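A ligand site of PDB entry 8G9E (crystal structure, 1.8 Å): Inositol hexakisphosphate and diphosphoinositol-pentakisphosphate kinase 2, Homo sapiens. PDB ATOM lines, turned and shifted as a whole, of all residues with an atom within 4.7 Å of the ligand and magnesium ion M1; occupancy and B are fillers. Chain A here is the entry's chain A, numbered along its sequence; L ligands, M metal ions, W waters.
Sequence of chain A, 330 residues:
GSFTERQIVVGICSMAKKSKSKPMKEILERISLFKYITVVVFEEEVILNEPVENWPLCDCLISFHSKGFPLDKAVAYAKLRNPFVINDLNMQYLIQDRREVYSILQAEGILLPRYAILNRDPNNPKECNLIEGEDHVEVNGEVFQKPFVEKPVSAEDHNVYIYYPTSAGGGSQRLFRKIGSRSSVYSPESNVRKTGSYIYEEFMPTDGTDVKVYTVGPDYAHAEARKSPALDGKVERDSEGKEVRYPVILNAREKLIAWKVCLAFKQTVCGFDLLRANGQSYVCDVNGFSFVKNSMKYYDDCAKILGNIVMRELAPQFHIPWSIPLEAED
The side-chain hydroxyl (OH) of Tyr 214 is in hydrogen-bond range of an oxygen (O21) of the ligand, 2.6 Å away.
NZ of Lys 242 is in salt-bridge range of O2 of the ligand.
NZ of Lys 178 lies within salt-bridge range of O4 of the ligand, at 2.7 Å.
NZ of Lys 18 lies within salt-bridge range of O18 of the ligand, 2.7 Å away.
O16 of the ligand sits at hydrogen-bond distance from OG of Ser 290 (2.7 Å).
NZ of Lys 293 lies within salt-bridge range of O17 of the ligand.
NZ of Lys 17 lies within salt-bridge range of O10 of the ligand, 2.9 Å away.
O2 of the ligand is in salt-bridge range of NH1 of Arg 237.
O25 of the ligand is in salt-bridge range of NH2 of Arg 226 (3.0 Å).
NH2 of Arg 177 is in salt-bridge range of O12 of the ligand (3.0 Å).
O22 of the ligand is in salt-bridge range of NZ of Lys 212, 3.4 Å away.
The side-chain hydroxyl (OG) of Ser 290 is in hydrogen-bond range of the side-chain amino group (NZ) of Lys 293, 3.3 Å away.
NZ of Lys 293 sits at hydrogen-bond distance from O of Phe 291.
The backbone carbonyl oxygen (O) of Gly 241 lies within hydrogen-bond range of the guanidinium group (NH1) of Arg 237 (2.7 Å).
NH1 of Arg 226 lies within salt-bridge range of OE1 of Glu 243 (3.1 Å).
NE2 of His 158 lies within hydrogen-bond range of NH2 of Arg 177.
11 residues have an atom within 4 Å of the ligand: Lys 17, Lys 18, Arg 177, Lys 178, Lys 212, Tyr 214, Arg 226, Arg 237, Lys 242, Ser 290 and Lys 293.
No residue comes within 4 Å of magnesium ion M1.
The nearest printed residue that does not touch magnesium ion M1 is Lys 178 (4.5 Å).
Magnesium ion M1 is bound by an oxygen (O9) of the ligand (2.0 Å), water W13 (2.0 Å), water W15 (2.1 Å), an oxygen (O5) of the ligand (2.1 Å), water W8 (2.1 Å) and water W5 (2.2 Å).
Magnesium ion M1 has six donor atoms within binding distance.
Water W5 bridges O of Lys 178 (2.7 Å) and O4 of the ligand (2.7 Å).
Water W7 lies within hydrogen-bond range of an oxygen (O18) of the ligand and the backbone carbonyl oxygen (O) of Phe 289.
Water W17 lies within hydrogen-bond range of an oxygen (O13) of the ligand (2.7 Å) and the side-chain amino group of Lys 17 (3.1 Å).
Water W11 lies within hydrogen-bond range of an oxygen (O17) of the ligand and the backbone NH of Phe 291.
Water W9 bridges NE2 of His 158 and O12 of the ligand.
Water W14 lies within hydrogen-bond range of O1 of the ligand and O of Lys 178.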
ATOM      1  N   LYS A  17      33.182  16.485   1.431  1.00  0.00           N
ATOM      2  CA  LYS A  17      31.828  17.000   1.653  1.00  0.00           C
ATOM      3  C   LYS A  17      30.750  16.051   1.102  1.00  0.00           C
ATOM      4  O   LYS A  17      29.590  16.017   1.570  1.00  0.00           O
ATOM      5  CB  LYS A  17      31.834  18.412   1.052  1.00  0.00           C
ATOM      6  CG  LYS A  17      30.537  18.982   0.537  1.00  0.00           C
ATOM      7  CD  LYS A  17      30.747  20.348  -0.051  1.00  0.00           C
ATOM      8  CE  LYS A  17      29.431  21.049  -0.219  1.00  0.00           C
ATOM      9  NZ  LYS A  17      29.605  22.406  -0.772  1.00  0.00           N
ATOM     10  N   LYS A  18      31.121  15.278   0.078  1.00  0.00           N
ATOM     11  CA  LYS A  18      30.228  14.298  -0.532  1.00  0.00           C
ATOM     12  C   LYS A  18      30.445  12.912   0.080  1.00  0.00           C
ATOM     13  O   LYS A  18      29.480  12.236   0.390  1.00  0.00           O
ATOM     14  CB  LYS A  18      30.421  14.281  -2.041  1.00  0.00           C
ATOM     15  CG  LYS A  18      30.363  15.631  -2.761  1.00  0.00           C
ATOM     16  CD  LYS A  18      29.082  16.406  -2.556  1.00  0.00           C
ATOM     17  CE  LYS A  18      29.031  17.677  -3.391  1.00  0.00           C
ATOM     18  NZ  LYS A  18      27.713  18.348  -3.262  1.00  0.00           N
ATOM     19  N   SER A  66      32.528  17.170  -8.124  1.00  0.00           N
ATOM     20  CA  SER A  66      31.843  18.313  -7.535  1.00  0.00           C
ATOM     21  C   SER A  66      32.875  19.424  -7.402  1.00  0.00           C
ATOM     22  O   SER A  66      34.028  19.205  -7.724  1.00  0.00           O
ATOM     23  CB  SER A  66      31.212  17.936  -6.206  1.00  0.00           C
ATOM     24  OG  SER A  66      32.198  17.533  -5.244  1.00  0.00           O
ATOM     25  N   HIS A 158      24.996  28.480 -10.505  1.00  0.00           N
ATOM     26  CA  HIS A 158      23.576  28.383 -10.190  1.00  0.00           C
ATOM     27  C   HIS A 158      22.874  29.737 -10.258  1.00  0.00           C
ATOM     28  O   HIS A 158      21.700  29.822  -9.877  1.00  0.00           O
ATOM     29  CB  HIS A 158      23.410  27.666  -8.828  1.00  0.00           C
ATOM     30  CG  HIS A 158      24.077  26.318  -8.873  1.00  0.00           C
ATOM     31  ND1 HIS A 158      23.645  25.351  -9.746  1.00  0.00           N
ATOM     32  CD2 HIS A 158      25.192  25.822  -8.271  1.00  0.00           C
ATOM     33  CE1 HIS A 158      24.417  24.275  -9.633  1.00  0.00           C
ATOM     34  NE2 HIS A 158      25.371  24.535  -8.741  1.00  0.00           N
ATOM     35  N   ARG A 177      22.284  29.056  -5.446  1.00  0.00           N
ATOM     36  CA  ARG A 177      22.385  27.967  -4.508  1.00  0.00           C
ATOM     37  C   ARG A 177      21.857  28.504  -3.171  1.00  0.00           C
ATOM     38  O   ARG A 177      22.243  29.581  -2.729  1.00  0.00           O
ATOM     39  CB  ARG A 177      23.807  27.410  -4.512  1.00  0.00           C
ATOM     40  CG  ARG A 177      24.053  26.342  -3.458  1.00  0.00           C
ATOM     41  CD  ARG A 177      23.258  25.042  -3.582  1.00  0.00           C
ATOM     42  NE  ARG A 177      23.695  24.160  -4.664  1.00  0.00           N
ATOM     43  CZ  ARG A 177      22.977  23.893  -5.765  1.00  0.00           C
ATOM     44  NH1 ARG A 177      21.828  24.497  -5.986  1.00  0.00           N
ATOM     45  NH2 ARG A 177      23.428  23.021  -6.649  1.00  0.00           N
ATOM     46  N   LYS A 178      20.932  27.762  -2.548  1.00  0.00           N
ATOM     47  CA  LYS A 178      20.147  28.351  -1.480  1.00  0.00           C
ATOM     48  C   LYS A 178      21.025  28.729  -0.290  1.00  0.00           C
ATOM     49  O   LYS A 178      22.047  28.088   0.033  1.00  0.00           O
ATOM     50  CB  LYS A 178      18.964  27.462  -1.101  1.00  0.00           C
ATOM     51  CG  LYS A 178      19.280  26.085  -0.582  1.00  0.00           C
ATOM     52  CD  LYS A 178      17.974  25.306  -0.427  1.00  0.00           C
ATOM     53  CE  LYS A 178      18.120  23.892   0.091  1.00  0.00           C
ATOM     54  NZ  LYS A 178      18.985  23.056  -0.777  1.00  0.00           N
ATOM     55  N   LYS A 212      12.307  16.484  -9.024  1.00  0.00           N
ATOM     56  CA  LYS A 212      13.709  16.090  -8.927  1.00  0.00           C
ATOM     57  C   LYS A 212      13.733  14.565  -8.989  1.00  0.00           C
ATOM     58  O   LYS A 212      12.993  13.890  -8.249  1.00  0.00           O
ATOM     59  CB  LYS A 212      14.317  16.588  -7.619  1.00  0.00           C
ATOM     60  CG  LYS A 212      14.082  18.049  -7.242  1.00  0.00           C
ATOM     61  CD  LYS A 212      15.205  18.936  -7.541  1.00  0.00           C
ATOM     62  CE  LYS A 212      16.332  18.887  -6.529  1.00  0.00           C
ATOM     63  NZ  LYS A 212      17.422  19.766  -7.011  1.00  0.00           N
ATOM     64  N   TYR A 214      16.008  10.910  -9.300  1.00  0.00           N
ATOM     65  CA  TYR A 214      17.247  10.311  -8.846  1.00  0.00           C
ATOM     66  C   TYR A 214      17.281   8.863  -9.295  1.00  0.00           C
ATOM     67  O   TYR A 214      16.491   8.054  -8.819  1.00  0.00           O
ATOM     68  CB  TYR A 214      17.316  10.400  -7.325  1.00  0.00           C
ATOM     69  CG  TYR A 214      17.301  11.789  -6.736  1.00  0.00           C
ATOM     70  CD1 TYR A 214      16.106  12.458  -6.506  1.00  0.00           C
ATOM     71  CD2 TYR A 214      18.480  12.400  -6.318  1.00  0.00           C
ATOM     72  CE1 TYR A 214      16.102  13.723  -5.929  1.00  0.00           C
ATOM     73  CE2 TYR A 214      18.476  13.651  -5.740  1.00  0.00           C
ATOM     74  CZ  TYR A 214      17.290  14.316  -5.524  1.00  0.00           C
ATOM     75  OH  TYR A 214      17.282  15.526  -4.900  1.00  0.00           O
ATOM     76  N   ARG A 226       9.667  19.783  -5.184  1.00  0.00           N
ATOM     77  CA  ARG A 226       9.937  20.897  -4.299  1.00  0.00           C
ATOM     78  C   ARG A 226       9.378  22.148  -4.930  1.00  0.00           C
ATOM     79  O   ARG A 226       9.233  22.201  -6.150  1.00  0.00           O
ATOM     80  CB  ARG A 226      11.443  21.118  -4.069  1.00  0.00           C
ATOM     81  CG  ARG A 226      12.050  19.918  -3.374  1.00  0.00           C
ATOM     82  CD  ARG A 226      13.472  20.139  -2.937  1.00  0.00           C
ATOM     83  NE  ARG A 226      14.128  18.905  -2.575  1.00  0.00           N
ATOM     84  CZ  ARG A 226      15.380  18.884  -2.157  1.00  0.00           C
ATOM     85  NH1 ARG A 226      15.949  20.014  -1.777  1.00  0.00           N
ATOM     86  NH2 ARG A 226      15.988  17.722  -2.007  1.00  0.00           N
ATOM     87  N   ARG A 237      10.964  25.078   4.945  1.00  0.00           N
ATOM     88  CA  ARG A 237      11.773  24.134   5.688  1.00  0.00           C
ATOM     89  C   ARG A 237      10.910  23.459   6.727  1.00  0.00           C
ATOM     90  O   ARG A 237      10.007  24.093   7.269  1.00  0.00           O
ATOM     91  CB  ARG A 237      12.971  24.821   6.349  1.00  0.00           C
ATOM     92  CG  ARG A 237      13.990  25.226   5.302  1.00  0.00           C
ATOM     93  CD  ARG A 237      15.370  25.526   5.822  1.00  0.00           C
ATOM     94  NE  ARG A 237      16.186  25.956   4.686  1.00  0.00           N
ATOM     95  CZ  ARG A 237      17.169  25.252   4.133  1.00  0.00           C
ATOM     96  NH1 ARG A 237      17.309  23.952   4.389  1.00  0.00           N
ATOM     97  NH2 ARG A 237      17.987  25.838   3.285  1.00  0.00           N
ATOM     98  N   GLY A 241      14.780  21.882   9.663  1.00  0.00           N
ATOM     99  CA  GLY A 241      15.742  22.604   8.850  1.00  0.00           C
ATOM    100  C   GLY A 241      15.888  22.042   7.441  1.00  0.00           C
ATOM    101  O   GLY A 241      16.708  22.542   6.668  1.00  0.00           O
ATOM    102  N   LYS A 242      15.098  21.021   7.080  1.00  0.00           N
ATOM    103  CA  LYS A 242      15.220  20.378   5.777  1.00  0.00           C
ATOM    104  C   LYS A 242      14.180  20.968   4.828  1.00  0.00           C
ATOM    105  O   LYS A 242      13.032  21.204   5.196  1.00  0.00           O
ATOM    106  CB  LYS A 242      15.065  18.859   5.902  1.00  0.00           C
ATOM    107  CG  LYS A 242      16.365  18.135   6.252  1.00  0.00           C
ATOM    108  CD  LYS A 242      17.501  18.407   5.231  1.00  0.00           C
ATOM    109  CE  LYS A 242      18.457  19.517   5.641  1.00  0.00           C
ATOM    110  NZ  LYS A 242      19.250  20.077   4.511  1.00  0.00           N
ATOM    111  N   GLU A 243      14.583  21.177   3.575  1.00  0.00           N
ATOM    112  CA  GLU A 243      13.634  21.697   2.614  1.00  0.00           C
ATOM    113  C   GLU A 243      12.476  20.706   2.459  1.00  0.00           C
ATOM    114  O   GLU A 243      12.704  19.513   2.313  1.00  0.00           O
ATOM    115  CB  GLU A 243      14.264  21.960   1.258  1.00  0.00           C
ATOM    116  CG  GLU A 243      13.257  22.660   0.341  1.00  0.00           C
ATOM    117  CD  GLU A 243      13.830  23.246  -0.935  1.00  0.00           C
ATOM    118  OE1 GLU A 243      14.936  22.857  -1.268  1.00  0.00           O
ATOM    119  OE2 GLU A 243      13.156  24.115  -1.578  1.00  0.00           O
ATOM    120  N   ARG A 245       9.686  18.535   0.835  1.00  0.00           N
ATOM    121  CA  ARG A 245       9.591  17.720  -0.371  1.00  0.00           C
ATOM    122  C   ARG A 245       8.162  17.173  -0.443  1.00  0.00           C
ATOM    123  O   ARG A 245       7.540  16.837   0.571  1.00  0.00           O
ATOM    124  CB  ARG A 245      10.591  16.545  -0.309  1.00  0.00           C
ATOM    125  CG  ARG A 245      12.075  16.907  -0.235  1.00  0.00           C
ATOM    126  CD  ARG A 245      12.877  16.510   1.024  1.00  0.00           C
ATOM    127  NE  ARG A 245      14.335  16.474   0.832  1.00  0.00           N
ATOM    128  CZ  ARG A 245      15.258  17.225   1.478  1.00  0.00           C
ATOM    129  NH1 ARG A 245      14.890  18.229   2.244  1.00  0.00           N
ATOM    130  NH2 ARG A 245      16.553  16.977   1.311  1.00  0.00           N
ATOM    131  N   ASN A 287      22.212  16.767 -13.416  1.00  0.00           N
ATOM    132  CA  ASN A 287      23.240  17.044 -12.413  1.00  0.00           C
ATOM    133  C   ASN A 287      24.296  15.946 -12.294  1.00  0.00           C
ATOM    134  O   ASN A 287      25.402  16.208 -11.798  1.00  0.00           O
ATOM    135  CB  ASN A 287      22.606  17.368 -11.072  1.00  0.00           C
ATOM    136  CG  ASN A 287      21.789  18.637 -11.181  1.00  0.00           C
ATOM    137  OD1 ASN A 287      20.677  18.714 -10.633  1.00  0.00           O
ATOM    138  ND2 ASN A 287      22.357  19.617 -11.874  1.00  0.00           N
ATOM    139  N   PHE A 289      25.861  12.622 -10.508  1.00  0.00           N
ATOM    140  CA  PHE A 289      25.792  11.896  -9.251  1.00  0.00           C
ATOM    141  C   PHE A 289      25.079  12.692  -8.139  1.00  0.00           C
ATOM    142  O   PHE A 289      25.489  13.766  -7.750  1.00  0.00           O
ATOM    143  CB  PHE A 289      27.189  11.492  -8.796  1.00  0.00           C
ATOM    144  CG  PHE A 289      27.182  10.411  -7.752  1.00  0.00           C
ATOM    145  CD1 PHE A 289      26.848  10.695  -6.432  1.00  0.00           C
ATOM    146  CD2 PHE A 289      27.478   9.095  -8.100  1.00  0.00           C
ATOM    147  CE1 PHE A 289      26.806   9.677  -5.498  1.00  0.00           C
ATOM    148  CE2 PHE A 289      27.478   8.097  -7.146  1.00  0.00           C
ATOM    149  CZ  PHE A 289      27.141   8.384  -5.847  1.00  0.00           C
ATOM    150  N   SER A 290      24.009  12.082  -7.611  1.00  0.00           N
ATOM    151  CA  SER A 290      23.236  12.661  -6.529  1.00  0.00           C
ATOM    152  C   SER A 290      22.417  11.542  -5.858  1.00  0.00           C
ATOM    153  O   SER A 290      21.768  10.725  -6.502  1.00  0.00           O
ATOM    154  CB  SER A 290      22.357  13.799  -6.997  1.00  0.00           C
ATOM    155  OG  SER A 290      21.810  14.476  -5.867  1.00  0.00           O
ATOM    156  N   PHE A 291      22.473  11.543  -4.529  1.00  0.00           N
ATOM    157  CA  PHE A 291      21.665  10.652  -3.730  1.00  0.00           C
ATOM    158  C   PHE A 291      20.447  11.423  -3.183  1.00  0.00           C
ATOM    159  O   PHE A 291      20.543  12.606  -2.871  1.00  0.00           O
ATOM    160  CB  PHE A 291      22.489  10.139  -2.552  1.00  0.00           C
ATOM    161  CG  PHE A 291      23.521   9.088  -2.860  1.00  0.00           C
ATOM    162  CD1 PHE A 291      23.334   8.151  -3.856  1.00  0.00           C
ATOM    163  CD2 PHE A 291      24.657   9.021  -2.092  1.00  0.00           C
ATOM    164  CE1 PHE A 291      24.283   7.167  -4.095  1.00  0.00           C
ATOM    165  CE2 PHE A 291      25.589   8.020  -2.304  1.00  0.00           C
ATOM    166  CZ  PHE A 291      25.393   7.083  -3.298  1.00  0.00           C
ATOM    167  N   LYS A 293      18.109  12.472  -0.203  1.00  0.00           N
ATOM    168  CA  LYS A 293      18.388  12.782   1.183  1.00  0.00           C
ATOM    169  C   LYS A 293      17.170  12.412   2.015  1.00  0.00           C
ATOM    170  O   LYS A 293      16.036  12.674   1.622  1.00  0.00           O
ATOM    171  CB  LYS A 293      18.670  14.282   1.343  1.00  0.00           C
ATOM    172  CG  LYS A 293      19.977  14.813   0.766  1.00  0.00           C
ATOM    173  CD  LYS A 293      19.996  14.896  -0.749  1.00  0.00           C
ATOM    174  CE  LYS A 293      21.203  15.616  -1.293  1.00  0.00           C
ATOM    175  NZ  LYS A 293      21.443  15.278  -2.722  1.00  0.00           N
HETATM  176  C1  LIG L   1      22.734  20.972  -1.618  1.00  0.00           C
HETATM  177  C2  LIG L   1      24.185  20.840  -2.044  1.00  0.00           C
HETATM  178  C3  LIG L   1      23.461  19.386  -3.946  1.00  0.00           C
HETATM  179  C4  LIG L   1      21.965  19.531  -3.480  1.00  0.00           C
HETATM  180  C5  LIG L   1      24.286  20.594  -3.525  1.00  0.00           C
HETATM  181  O1  LIG L   1      20.531  24.531   2.531  1.00  0.00           O
HETATM  182  P1  LIG L   1      20.967  23.349   3.396  1.00  0.00           P
HETATM  183  O2  LIG L   1      19.870  22.574   4.083  1.00  0.00           O
HETATM  184  O3  LIG L   1      22.339  23.432   4.062  1.00  0.00           O
HETATM  185  C6  LIG L   1      21.336  21.928   2.007  1.00  0.00           C
HETATM  186  F1  LIG L   1      20.208  21.551   1.399  1.00  0.00           F
HETATM  187  F2  LIG L   1      21.964  20.826   2.572  1.00  0.00           F
HETATM  188  P2  LIG L   1      22.403  22.537   0.580  1.00  0.00           P
HETATM  189  O4  LIG L   1      21.600  23.448  -0.368  1.00  0.00           O
HETATM  190  O5  LIG L   1      23.750  22.980   1.177  1.00  0.00           O
HETATM  191  O6  LIG L   1      22.659  21.086  -0.193  1.00  0.00           O
HETATM  192  O7  LIG L   1      24.655  22.175  -1.852  1.00  0.00           O
HETATM  193  P3  LIG L   1      26.064  22.582  -1.081  1.00  0.00           P
HETATM  194  O8  LIG L   1      26.391  21.436  -0.115  1.00  0.00           O
HETATM  195  O9  LIG L   1      25.780  23.941  -0.474  1.00  0.00           O
HETATM  196  O10 LIG L   1      27.126  22.718  -2.232  1.00  0.00           O
HETATM  197  O11 LIG L   1      25.670  20.346  -3.862  1.00  0.00           O
HETATM  198  P4  LIG L   1      26.415  21.248  -4.997  1.00  0.00           P
HETATM  199  O12 LIG L   1      25.617  21.005  -6.252  1.00  0.00           O
HETATM  200  O13 LIG L   1      27.875  20.645  -4.953  1.00  0.00           O
HETATM  201  O14 LIG L   1      26.325  22.673  -4.434  1.00  0.00           O
HETATM  202  O15 LIG L   1      24.000  18.259  -3.301  1.00  0.00           O
HETATM  203  P5  LIG L   1      24.334  16.855  -4.078  1.00  0.00           P
HETATM  204  O16 LIG L   1      23.341  16.651  -5.195  1.00  0.00           O
HETATM  205  O17 LIG L   1      24.182  15.917  -2.965  1.00  0.00           O
HETATM  206  O18 LIG L   1      25.774  16.995  -4.550  1.00  0.00           O
HETATM  207  O19 LIG L   1      21.318  18.248  -3.625  1.00  0.00           O
HETATM  208  P6  LIG L   1      20.045  18.044  -4.642  1.00  0.00           P
HETATM  209  O20 LIG L   1      20.670  18.612  -5.986  1.00  0.00           O
HETATM  210  O21 LIG L   1      19.605  16.587  -4.690  1.00  0.00           O
HETATM  211  O22 LIG L   1      18.911  18.928  -4.056  1.00  0.00           O
HETATM  212  C7  LIG L   1      21.850  19.816  -2.020  1.00  0.00           C
HETATM  213  O23 LIG L   1      20.501  20.250  -1.696  1.00  0.00           O
HETATM  214  P7  LIG L   1      19.463  19.257  -0.739  1.00  0.00           P
HETATM  215  O24 LIG L   1      20.245  18.560   0.393  1.00  0.00           O
HETATM  216  O25 LIG L   1      18.885  18.415  -1.786  1.00  0.00           O
HETATM  217  O26 LIG L   1      18.500  20.319  -0.202  1.00  0.00           O
HETATM  218 MG    MG M   1      24.808  24.752   1.072  1.00  0.00          MG
HETATM  219 MG    MG M   2      26.821  17.920  -8.652  1.00  0.00          MG
HETATM  220  O   HOH W   1      27.333  26.014  -1.563  1.00  0.00           O
HETATM  221  O   HOH W   2      24.385  21.847   4.114  1.00  0.00           O
HETATM  222  O   HOH W   3      26.135  18.647  -6.935  1.00  0.00           O
HETATM  223  O   HOH W   4      22.866  17.449  -7.554  1.00  0.00           O
HETATM  224  O   HOH W   5      23.194  25.646  -0.151  1.00  0.00           O
HETATM  225  O   HOH W   6      22.725  18.073   1.430  1.00  0.00           O
HETATM  226  O   HOH W   7      27.107  15.185  -5.790  1.00  0.00           O
HETATM  227  O   HOH W   8      23.846  25.335   2.816  1.00  0.00           O
HETATM  228  O   HOH W   9      26.887  22.306  -8.358  1.00  0.00           O
HETATM  229  O   HOH W  10      17.256  20.505   2.200  1.00  0.00           O
HETATM  230  O   HOH W  11      24.538  13.179  -3.153  1.00  0.00           O
HETATM  231  O   HOH W  12      27.536  24.883  -5.661  1.00  0.00           O
HETATM  232  O   HOH W  13      26.333  23.943   2.159  1.00  0.00           O
HETATM  233  O   HOH W  14      21.833  27.200   3.387  1.00  0.00           O
HETATM  234  O   HOH W  15      25.770  26.578   1.005  1.00  0.00           O
HETATM  235  O   HOH W  16      29.538  20.960  -6.990  1.00  0.00           O
HETATM  236  O   HOH W  17      30.193  21.046  -3.536  1.00  0.00           O
HETATM  237  O   HOH W  18      23.566  20.459  -8.704  1.00  0.00           O
